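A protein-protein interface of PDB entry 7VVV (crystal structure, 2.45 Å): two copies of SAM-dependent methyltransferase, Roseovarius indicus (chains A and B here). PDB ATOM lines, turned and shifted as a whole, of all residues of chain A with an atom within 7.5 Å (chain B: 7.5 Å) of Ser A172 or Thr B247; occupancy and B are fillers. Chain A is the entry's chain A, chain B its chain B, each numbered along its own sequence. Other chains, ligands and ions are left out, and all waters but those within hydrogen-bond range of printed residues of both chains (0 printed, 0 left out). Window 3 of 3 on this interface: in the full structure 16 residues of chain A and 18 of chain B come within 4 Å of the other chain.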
ATOM      1  N   VAL A 125      -9.334   2.367  18.039  1.00  0.00           N
ATOM      2  CA  VAL A 125     -10.727   2.055  18.325  1.00  0.00           C
ATOM      3  C   VAL A 125     -11.402   1.494  17.077  1.00  0.00           C
ATOM      4  O   VAL A 125     -11.384   2.113  16.005  1.00  0.00           O
ATOM      5  CB  VAL A 125     -11.452   3.313  18.826  1.00  0.00           C
ATOM      6  CG1 VAL A 125     -12.931   3.000  19.078  1.00  0.00           C
ATOM      7  CG2 VAL A 125     -10.769   3.857  20.064  1.00  0.00           C
ATOM      8  N   TRP A 162      -2.028   4.047  26.506  1.00  0.00           N
ATOM      9  CA  TRP A 162      -2.941   4.888  25.826  1.00  0.00           C
ATOM     10  C   TRP A 162      -3.069   6.294  26.341  1.00  0.00           C
ATOM     11  O   TRP A 162      -3.491   7.121  25.632  1.00  0.00           O
ATOM     12  CB  TRP A 162      -4.295   4.220  25.969  1.00  0.00           C
ATOM     13  CG  TRP A 162      -4.592   4.119  27.369  1.00  0.00           C
ATOM     14  CD1 TRP A 162      -4.008   3.289  28.251  1.00  0.00           C
ATOM     15  CD2 TRP A 162      -5.412   4.984  28.110  1.00  0.00           C
ATOM     16  NE1 TRP A 162      -4.459   3.541  29.488  1.00  0.00           N
ATOM     17  CE2 TRP A 162      -5.327   4.593  29.433  1.00  0.00           C
ATOM     18  CE3 TRP A 162      -6.232   6.040  27.780  1.00  0.00           C
ATOM     19  CZ2 TRP A 162      -6.043   5.218  30.433  1.00  0.00           C
ATOM     20  CZ3 TRP A 162      -6.939   6.656  28.768  1.00  0.00           C
ATOM     21  CH2 TRP A 162      -6.845   6.247  30.078  1.00  0.00           C
ATOM     22  N   PHE A 165      -1.408   9.305  24.416  1.00  0.00           N
ATOM     23  CA  PHE A 165      -1.944   9.601  23.095  1.00  0.00           C
ATOM     24  C   PHE A 165      -3.355  10.151  23.156  1.00  0.00           C
ATOM     25  O   PHE A 165      -3.984  10.341  22.113  1.00  0.00           O
ATOM     26  CB  PHE A 165      -1.875   8.363  22.205  1.00  0.00           C
ATOM     27  CG  PHE A 165      -0.555   7.663  22.288  1.00  0.00           C
ATOM     28  CD1 PHE A 165       0.611   8.296  21.862  1.00  0.00           C
ATOM     29  CD2 PHE A 165      -0.447   6.409  22.871  1.00  0.00           C
ATOM     30  CE1 PHE A 165       1.856   7.666  21.961  1.00  0.00           C
ATOM     31  CE2 PHE A 165       0.810   5.781  22.980  1.00  0.00           C
ATOM     32  CZ  PHE A 165       1.951   6.408  22.522  1.00  0.00           C
ATOM     33  N   ASP A 166      -3.838  10.475  24.351  1.00  0.00           N
ATOM     34  CA  ASP A 166      -5.236  10.842  24.523  1.00  0.00           C
ATOM     35  C   ASP A 166      -5.520  12.257  24.045  1.00  0.00           C
ATOM     36  O   ASP A 166      -6.643  12.549  23.624  1.00  0.00           O
ATOM     37  CB  ASP A 166      -5.627  10.684  25.999  1.00  0.00           C
ATOM     38  CG  ASP A 166      -7.120  10.888  26.248  1.00  0.00           C
ATOM     39  OD1 ASP A 166      -7.930  10.105  25.704  1.00  0.00           O
ATOM     40  OD2 ASP A 166      -7.485  11.814  27.011  1.00  0.00           O
ATOM     41  N   SER A 167      -4.535  13.147  24.121  1.00  0.00           N
ATOM     42  CA  SER A 167      -4.762  14.549  23.830  1.00  0.00           C
ATOM     43  C   SER A 167      -4.761  14.835  22.336  1.00  0.00           C
ATOM     44  O   SER A 167      -5.179  15.929  21.937  1.00  0.00           O
ATOM     45  CB  SER A 167      -3.691  15.415  24.520  1.00  0.00           C
ATOM     46  OG  SER A 167      -2.481  15.495  23.764  1.00  0.00           O
ATOM     47  N   TYR A 168      -4.296  13.885  21.528  1.00  0.00           N
ATOM     48  CA  TYR A 168      -4.181  14.082  20.095  1.00  0.00           C
ATOM     49  C   TYR A 168      -5.527  14.463  19.486  1.00  0.00           C
ATOM     50  O   TYR A 168      -6.555  13.852  19.813  1.00  0.00           O
ATOM     51  CB  TYR A 168      -3.641  12.820  19.427  1.00  0.00           C
ATOM     52  CG  TYR A 168      -2.149  12.738  19.511  1.00  0.00           C
ATOM     53  CD1 TYR A 168      -1.349  13.361  18.563  1.00  0.00           C
ATOM     54  CD2 TYR A 168      -1.522  12.054  20.553  1.00  0.00           C
ATOM     55  CE1 TYR A 168       0.051  13.315  18.645  1.00  0.00           C
ATOM     56  CE2 TYR A 168      -0.126  11.983  20.637  1.00  0.00           C
ATOM     57  CZ  TYR A 168       0.651  12.629  19.675  1.00  0.00           C
ATOM     58  OH  TYR A 168       2.025  12.582  19.734  1.00  0.00           O
ATOM     59  N   PRO A 169      -5.555  15.476  18.609  1.00  0.00           N
ATOM     60  CA  PRO A 169      -6.806  15.830  17.908  1.00  0.00           C
ATOM     61  C   PRO A 169      -7.576  14.651  17.325  1.00  0.00           C
ATOM     62  O   PRO A 169      -8.791  14.576  17.518  1.00  0.00           O
ATOM     63  CB  PRO A 169      -6.313  16.777  16.806  1.00  0.00           C
ATOM     64  CG  PRO A 169      -5.139  17.460  17.413  1.00  0.00           C
ATOM     65  CD  PRO A 169      -4.457  16.410  18.288  1.00  0.00           C
ATOM     66  N   PHE A 170      -6.909  13.726  16.632  1.00  0.00           N
ATOM     67  CA  PHE A 170      -7.609  12.610  16.007  1.00  0.00           C
ATOM     68  C   PHE A 170      -7.857  11.448  16.959  1.00  0.00           C
ATOM     69  O   PHE A 170      -8.345  10.396  16.521  1.00  0.00           O
ATOM     70  CB  PHE A 170      -6.835  12.144  14.776  1.00  0.00           C
ATOM     71  CG  PHE A 170      -7.052  13.033  13.589  1.00  0.00           C
ATOM     72  CD1 PHE A 170      -6.262  14.160  13.405  1.00  0.00           C
ATOM     73  CD2 PHE A 170      -8.085  12.787  12.685  1.00  0.00           C
ATOM     74  CE1 PHE A 170      -6.475  15.018  12.320  1.00  0.00           C
ATOM     75  CE2 PHE A 170      -8.296  13.657  11.591  1.00  0.00           C
ATOM     76  CZ  PHE A 170      -7.493  14.765  11.423  1.00  0.00           C
ATOM     77  N   ASN A 171      -7.539  11.601  18.244  1.00  0.00           N
ATOM     78  CA  ASN A 171      -8.004  10.616  19.199  1.00  0.00           C
ATOM     79  C   ASN A 171      -9.506  10.707  19.392  1.00  0.00           C
ATOM     80  O   ASN A 171     -10.112   9.764  19.888  1.00  0.00           O
ATOM     81  CB  ASN A 171      -7.299  10.784  20.542  1.00  0.00           C
ATOM     82  CG  ASN A 171      -7.387   9.534  21.387  1.00  0.00           C
ATOM     83  OD1 ASN A 171      -7.087   8.430  20.914  1.00  0.00           O
ATOM     84  ND2 ASN A 171      -7.855   9.688  22.625  1.00  0.00           N
ATOM     85  N   SER A 172     -10.122  11.818  18.992  1.00  0.00           N
ATOM     86  CA  SER A 172     -11.568  11.955  19.103  1.00  0.00           C
ATOM     87  C   SER A 172     -12.319  11.031  18.150  1.00  0.00           C
ATOM     88  O   SER A 172     -13.500  10.748  18.385  1.00  0.00           O
ATOM     89  CB  SER A 172     -11.956  13.396  18.832  1.00  0.00           C
ATOM     90  OG  SER A 172     -11.512  13.729  17.532  1.00  0.00           O
ATOM     91  N   VAL A 173     -11.678  10.561  17.085  1.00  0.00           N
ATOM     92  CA  VAL A 173     -12.251   9.514  16.247  1.00  0.00           C
ATOM     93  C   VAL A 173     -11.484   8.202  16.416  1.00  0.00           C
ATOM     94  O   VAL A 173     -11.564   7.323  15.562  1.00  0.00           O
ATOM     95  CB  VAL A 173     -12.329   9.941  14.766  1.00  0.00           C
ATOM     96  CG1 VAL A 173     -13.232  11.162  14.597  1.00  0.00           C
ATOM     97  CG2 VAL A 173     -10.936  10.216  14.199  1.00  0.00           C
ATOM     98  N   GLY A 174     -10.737   8.061  17.517  1.00  0.00           N
ATOM     99  CA  GLY A 174     -10.116   6.796  17.871  1.00  0.00           C
ATOM    100  C   GLY A 174      -8.798   6.460  17.196  1.00  0.00           C
ATOM    101  O   GLY A 174      -8.417   5.281  17.163  1.00  0.00           O
ATOM    102  N   LEU A 175      -8.077   7.454  16.664  1.00  0.00           N
ATOM    103  CA  LEU A 175      -6.857   7.218  15.900  1.00  0.00           C
ATOM    104  C   LEU A 175      -5.684   8.006  16.475  1.00  0.00           C
ATOM    105  O   LEU A 175      -4.750   8.370  15.746  1.00  0.00           O
ATOM    106  CB  LEU A 175      -7.055   7.578  14.430  1.00  0.00           C
ATOM    107  CG  LEU A 175      -8.262   6.980  13.696  1.00  0.00           C
ATOM    108  CD1 LEU A 175      -8.526   7.762  12.415  1.00  0.00           C
ATOM    109  CD2 LEU A 175      -8.037   5.506  13.393  1.00  0.00           C
ATOM    110  N   GLY A 176      -5.731   8.241  17.751  1.00  0.00           N
ATOM    111  CA  GLY A 176      -4.686   8.957  18.392  1.00  0.00           C
ATOM    112  C   GLY A 176      -3.323   8.381  18.237  1.00  0.00           C
ATOM    113  O   GLY A 176      -2.415   9.087  18.119  1.00  0.00           O
ATOM    114  N   GLU A 179      -1.971   9.067  14.781  1.00  0.00           N
ATOM    115  CA  GLU A 179      -1.576  10.453  14.564  1.00  0.00           C
ATOM    116  C   GLU A 179      -0.178  10.653  15.119  1.00  0.00           C
ATOM    117  O   GLU A 179       0.673  11.288  14.497  1.00  0.00           O
ATOM    118  CB  GLU A 179      -2.558  11.407  15.245  1.00  0.00           C
ATOM    119  CG  GLU A 179      -2.288  12.877  14.971  1.00  0.00           C
ATOM    120  CD  GLU A 179      -3.396  13.777  15.480  1.00  0.00           C
ATOM    121  OE1 GLU A 179      -3.399  14.976  15.128  1.00  0.00           O
ATOM    122  OE2 GLU A 179      -4.264  13.287  16.232  1.00  0.00           O
ATOM    123  N   VAL A 202     -15.263   5.695  10.548  1.00  0.00           N
ATOM    124  CA  VAL A 202     -15.350   7.115  10.770  1.00  0.00           C
ATOM    125  C   VAL A 202     -15.487   7.897   9.507  1.00  0.00           C
ATOM    126  O   VAL A 202     -15.818   9.016   9.517  1.00  0.00           O
ATOM    127  CB  VAL A 202     -14.238   7.672  11.675  1.00  0.00           C
ATOM    128  CG1 VAL A 202     -14.413   7.177  13.070  1.00  0.00           C
ATOM    129  CG2 VAL A 202     -12.871   7.338  11.188  1.00  0.00           C
ATOM    130  N   VAL A 206     -12.462  11.720   7.042  1.00  0.00           N
ATOM    131  CA  VAL A 206     -11.745  11.860   8.307  1.00  0.00           C
ATOM    132  C   VAL A 206     -10.381  11.188   8.231  1.00  0.00           C
ATOM    133  O   VAL A 206      -9.366  11.767   8.639  1.00  0.00           O
ATOM    134  CB  VAL A 206     -12.592  11.294   9.459  1.00  0.00           C
ATOM    135  CG1 VAL A 206     -11.706  10.955  10.653  1.00  0.00           C
ATOM    136  CG2 VAL A 206     -13.656  12.302   9.840  1.00  0.00           C
ATOM    137  N   PHE A 236     -19.229   3.506  20.741  1.00  0.00           N
ATOM    138  CA  PHE A 236     -18.307   4.599  20.468  1.00  0.00           C
ATOM    139  C   PHE A 236     -18.712   5.335  19.195  1.00  0.00           C
ATOM    140  O   PHE A 236     -18.894   6.555  19.202  1.00  0.00           O
ATOM    141  CB  PHE A 236     -16.874   4.078  20.351  1.00  0.00           C
ATOM    142  CG  PHE A 236     -15.890   5.135  19.928  1.00  0.00           C
ATOM    143  CD1 PHE A 236     -15.274   5.943  20.872  1.00  0.00           C
ATOM    144  CD2 PHE A 236     -15.607   5.346  18.580  1.00  0.00           C
ATOM    145  CE1 PHE A 236     -14.377   6.926  20.476  1.00  0.00           C
ATOM    146  CE2 PHE A 236     -14.723   6.325  18.185  1.00  0.00           C
ATOM    147  CZ  PHE A 236     -14.108   7.117  19.132  1.00  0.00           C
ATOM    148  N   ALA A 239     -21.864   7.134  19.580  1.00  0.00           N
ATOM    149  CA  ALA A 239     -21.663   8.344  20.369  1.00  0.00           C
ATOM    150  C   ALA A 239     -21.143   9.490  19.511  1.00  0.00           C
ATOM    151  O   ALA A 239     -21.488  10.654  19.759  1.00  0.00           O
ATOM    152  CB  ALA A 239     -20.713   8.046  21.537  1.00  0.00           C
ATOM    153  N   LEU A 240     -20.329   9.185  18.490  1.00  0.00           N
ATOM    154  CA  LEU A 240     -19.896  10.221  17.550  1.00  0.00           C
ATOM    155  C   LEU A 240     -21.070  10.833  16.792  1.00  0.00           C
ATOM    156  O   LEU A 240     -21.015  12.011  16.423  1.00  0.00           O
ATOM    157  CB  LEU A 240     -18.891   9.655  16.541  1.00  0.00           C
ATOM    158  CG  LEU A 240     -17.529   9.184  17.034  1.00  0.00           C
ATOM    159  CD1 LEU A 240     -16.786   8.553  15.864  1.00  0.00           C
ATOM    160  CD2 LEU A 240     -16.766  10.362  17.619  1.00  0.00           C
ATOM    161  N   ALA A 243     -22.904  13.481  19.022  1.00  0.00           N
ATOM    162  CA  ALA A 243     -22.103  14.514  19.582  1.00  0.00           C
ATOM    163  C   ALA A 243     -22.236  15.820  18.881  1.00  0.00           C
ATOM    164  O   ALA A 243     -22.593  15.882  17.732  1.00  0.00           O
ATOM    165  CB  ALA A 243     -20.668  14.095  19.551  1.00  0.00           C
ATOM    166  N   ARG A 251     -23.525  19.239  15.102  1.00  0.00           N
ATOM    167  CA  ARG A 251     -22.557  18.581  14.235  1.00  0.00           C
ATOM    168  C   ARG A 251     -23.271  17.558  13.362  1.00  0.00           C
ATOM    169  O   ARG A 251     -24.058  16.745  13.865  1.00  0.00           O
ATOM    170  CB  ARG A 251     -21.474  17.898  15.076  1.00  0.00           C
ATOM    171  CG  ARG A 251     -20.506  17.003  14.324  1.00  0.00           C
ATOM    172  CD  ARG A 251     -20.046  15.861  15.227  1.00  0.00           C
ATOM    173  NE  ARG A 251     -18.600  15.657  15.156  1.00  0.00           N
ATOM    174  CZ  ARG A 251     -17.944  14.689  15.791  1.00  0.00           C
ATOM    175  NH1 ARG A 251     -16.623  14.588  15.667  1.00  0.00           N
ATOM    176  NH2 ARG A 251     -18.608  13.814  16.542  1.00  0.00           N
ATOM    177  N   PHE A 253     -22.795  14.308  11.350  1.00  0.00           N
ATOM    178  CA  PHE A 253     -21.866  13.245  11.109  1.00  0.00           C
ATOM    179  C   PHE A 253     -22.445  11.848  11.038  1.00  0.00           C
ATOM    180  O   PHE A 253     -23.333  11.514  11.761  1.00  0.00           O
ATOM    181  CB  PHE A 253     -20.876  13.315  12.214  1.00  0.00           C
ATOM    182  CG  PHE A 253     -19.843  12.320  12.114  1.00  0.00           C
ATOM    183  CD1 PHE A 253     -19.130  12.202  10.979  1.00  0.00           C
ATOM    184  CD2 PHE A 253     -19.630  11.477  13.118  1.00  0.00           C
ATOM    185  CE1 PHE A 253     -18.163  11.274  10.874  1.00  0.00           C
ATOM    186  CE2 PHE A 253     -18.675  10.541  13.025  1.00  0.00           C
ATOM    187  CZ  PHE A 253     -17.939  10.434  11.907  1.00  0.00           C
ATOM    188  N   LEU B 244     -12.744  10.966  31.794  1.00  0.00           N
ATOM    189  CA  LEU B 244     -12.994  10.031  30.748  1.00  0.00           C
ATOM    190  C   LEU B 244     -11.963  10.449  29.753  1.00  0.00           C
ATOM    191  O   LEU B 244     -11.383  11.511  29.911  1.00  0.00           O
ATOM    192  CB  LEU B 244     -14.349  10.285  30.165  1.00  0.00           C
ATOM    193  CG  LEU B 244     -15.096   9.033  29.804  1.00  0.00           C
ATOM    194  CD1 LEU B 244     -16.360   9.013  30.649  1.00  0.00           C
ATOM    195  CD2 LEU B 244     -15.417   9.132  28.331  1.00  0.00           C
ATOM    196  N   ALA B 245     -11.718   9.631  28.745  1.00  0.00           N
ATOM    197  CA  ALA B 245     -10.731   9.957  27.754  1.00  0.00           C
ATOM    198  C   ALA B 245     -11.014  11.297  27.034  1.00  0.00           C
ATOM    199  O   ALA B 245     -10.846  12.379  27.596  1.00  0.00           O
ATOM    200  CB  ALA B 245     -10.612   8.802  26.773  1.00  0.00           C
ATOM    201  N   GLN B 246     -11.435  11.164  25.801  1.00  0.00           N
ATOM    202  CA  GLN B 246     -11.796  12.241  24.904  1.00  0.00           C
ATOM    203  C   GLN B 246     -12.483  11.598  23.710  1.00  0.00           C
ATOM    204  O   GLN B 246     -13.185  12.244  22.964  1.00  0.00           O
ATOM    205  CB  GLN B 246     -10.564  13.050  24.509  1.00  0.00           C
ATOM    206  CG  GLN B 246     -10.003  13.826  25.683  1.00  0.00           C
ATOM    207  CD  GLN B 246      -9.026  14.915  25.292  1.00  0.00           C
ATOM    208  OE1 GLN B 246      -8.195  14.720  24.423  1.00  0.00           O
ATOM    209  NE2 GLN B 246      -9.115  16.073  25.956  1.00  0.00           N
ATOM    210  N   THR B 247     -12.267  10.298  23.562  1.00  0.00           N
ATOM    211  CA  THR B 247     -12.826   9.488  22.548  1.00  0.00           C
ATOM    212  C   THR B 247     -14.320   9.733  22.545  1.00  0.00           C
ATOM    213  O   THR B 247     -14.853  10.165  21.529  1.00  0.00           O
ATOM    214  CB  THR B 247     -12.455   8.026  22.833  1.00  0.00           C
ATOM    215  OG1 THR B 247     -11.997   7.912  24.172  1.00  0.00           O
ATOM    216  CG2 THR B 247     -11.318   7.624  21.995  1.00  0.00           C
ATOM    217  N   GLY B 248     -14.993   9.463  23.665  1.00  0.00           N
ATOM    218  CA  GLY B 248     -14.381   8.940  24.880  1.00  0.00           C
ATOM    219  C   GLY B 248     -14.780   7.581  25.488  1.00  0.00           C
ATOM    220  O   GLY B 248     -15.952   7.275  25.613  1.00  0.00           O
ATOM    221  N   LEU B 249     -13.775   6.791  25.883  1.00  0.00           N
ATOM    222  CA  LEU B 249     -13.908   5.475  26.516  1.00  0.00           C
ATOM    223  C   LEU B 249     -12.780   5.200  27.558  1.00  0.00           C
ATOM    224  O   LEU B 249     -11.618   5.464  27.309  1.00  0.00           O
ATOM    225  CB  LEU B 249     -14.032   4.357  25.464  1.00  0.00           C
ATOM    226  CG  LEU B 249     -12.861   3.858  24.639  1.00  0.00           C
ATOM    227  CD1 LEU B 249     -13.166   2.509  24.027  1.00  0.00           C
ATOM    228  CD2 LEU B 249     -12.480   4.832  23.564  1.00  0.00           C
ATOM    229  N   GLU B 250     -13.164   4.665  28.708  1.00  0.00           N
ATOM    230  CA  GLU B 250     -12.244   4.293  29.761  1.00  0.00           C
ATOM    231  C   GLU B 250     -11.281   5.380  30.228  1.00  0.00           C
ATOM    232  O   GLU B 250     -11.445   6.555  29.943  1.00  0.00           O
ATOM    233  CB  GLU B 250     -11.409   3.100  29.274  1.00  0.00           C
ATOM    234  CG  GLU B 250     -10.270   3.501  28.342  1.00  0.00           C
ATOM    235  CD  GLU B 250      -8.897   2.924  28.682  1.00  0.00           C
ATOM    236  OE1 GLU B 250      -8.735   2.233  29.695  1.00  0.00           O
ATOM    237  OE2 GLU B 250      -7.959   3.150  27.901  1.00  0.00           O
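O of Asp A166 lies close to OE1 of Gln B246, at 2.8 Å. The side-chain carboxylate (OD2) of Asp A166 lies close to the backbone carbonyl oxygen (O) of Ala B245, at 3.5 Å. The backbone carbonyl oxygen (O) of Thr B247 lies close to the backbone carbonyl oxygen (O) of Ser A172 (3.5 Å).
The side-chain amide nitrogen (ND2) of Asn A171 is in hydrogen-bond range of the side-chain carboxylate (OD1) of Asp A166, 3.1 Å away. O of Pro A169 sits at hydrogen-bond distance from OG of Ser A172, 2.8 Å away. The side-chain amide oxygen (OD1) of Asn A171 sits at hydrogen-bond distance from the backbone NH (N) of Gly A176 (3.4 Å). The backbone NH (N) of Ala B245 lies within hydrogen-bond range of the backbone carbonyl oxygen (O) of Glu B250, at 3.3 Å. N of Leu B249 lies within hydrogen-bond range of OG1 of Thr B247 (2.7 Å).
OE2 of Glu B250 touches CD2 of Trp A162 (3.1 Å). Gln B246 touches Ser A167. Asn A171 touches Thr B247. Phe A236 touches Thr B247 (CE1 to CB, 3.2 Å).
Ser A172 touches one residue of chain B. Of chain A, only Asn A171, Ser A172 and Phe A236 come within 4 Å of Thr B247. Of the printed residues of chain B, Phe A236 touches Thr B247. Of the printed residues of chain B, Asp A166 touches Ala B245 and Gln B246. Of the printed residues of chain A, Ala B245 touches Asp A166 (3.2 Å). Of the printed residues of chain A, Gln B246 touches Asp A166 and Ser A167. Printed residues of chain B within 4 Å of Trp A162: Glu B250 (3.1 Å). Arg A251 touches none of the printed residues of chain B. The nearest residue of chain B that does not touch Ser A172 is Gln B246 (4.2 Å). The nearest printed residue of chain B that does not touch Asp A166 is Thr B247 (4.8 Å).
Printed residues of chain B that touch a printed residue of chain A: Ala B245, Gln B246, Thr B247 and Glu B250. Hydrophobic or aromatic side chains of chain B within 4 Å of the printed part of chain A: Ala B245. Along chain B the printed residues that touch a printed residue of chain A span positions 245 to 250. Of the 23 printed residues of chain A, 6 touch a printed residue of chain B. Among the printed residues, no Asp or Glu carboxylate lies within 4 Å of a Lys or Arg side-chain nitrogen of the other chain.
No position is printed for both chains. Of the 7 pairs that touch across the chains among the printed residues, none has its exchanged pair printed and touching as well.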
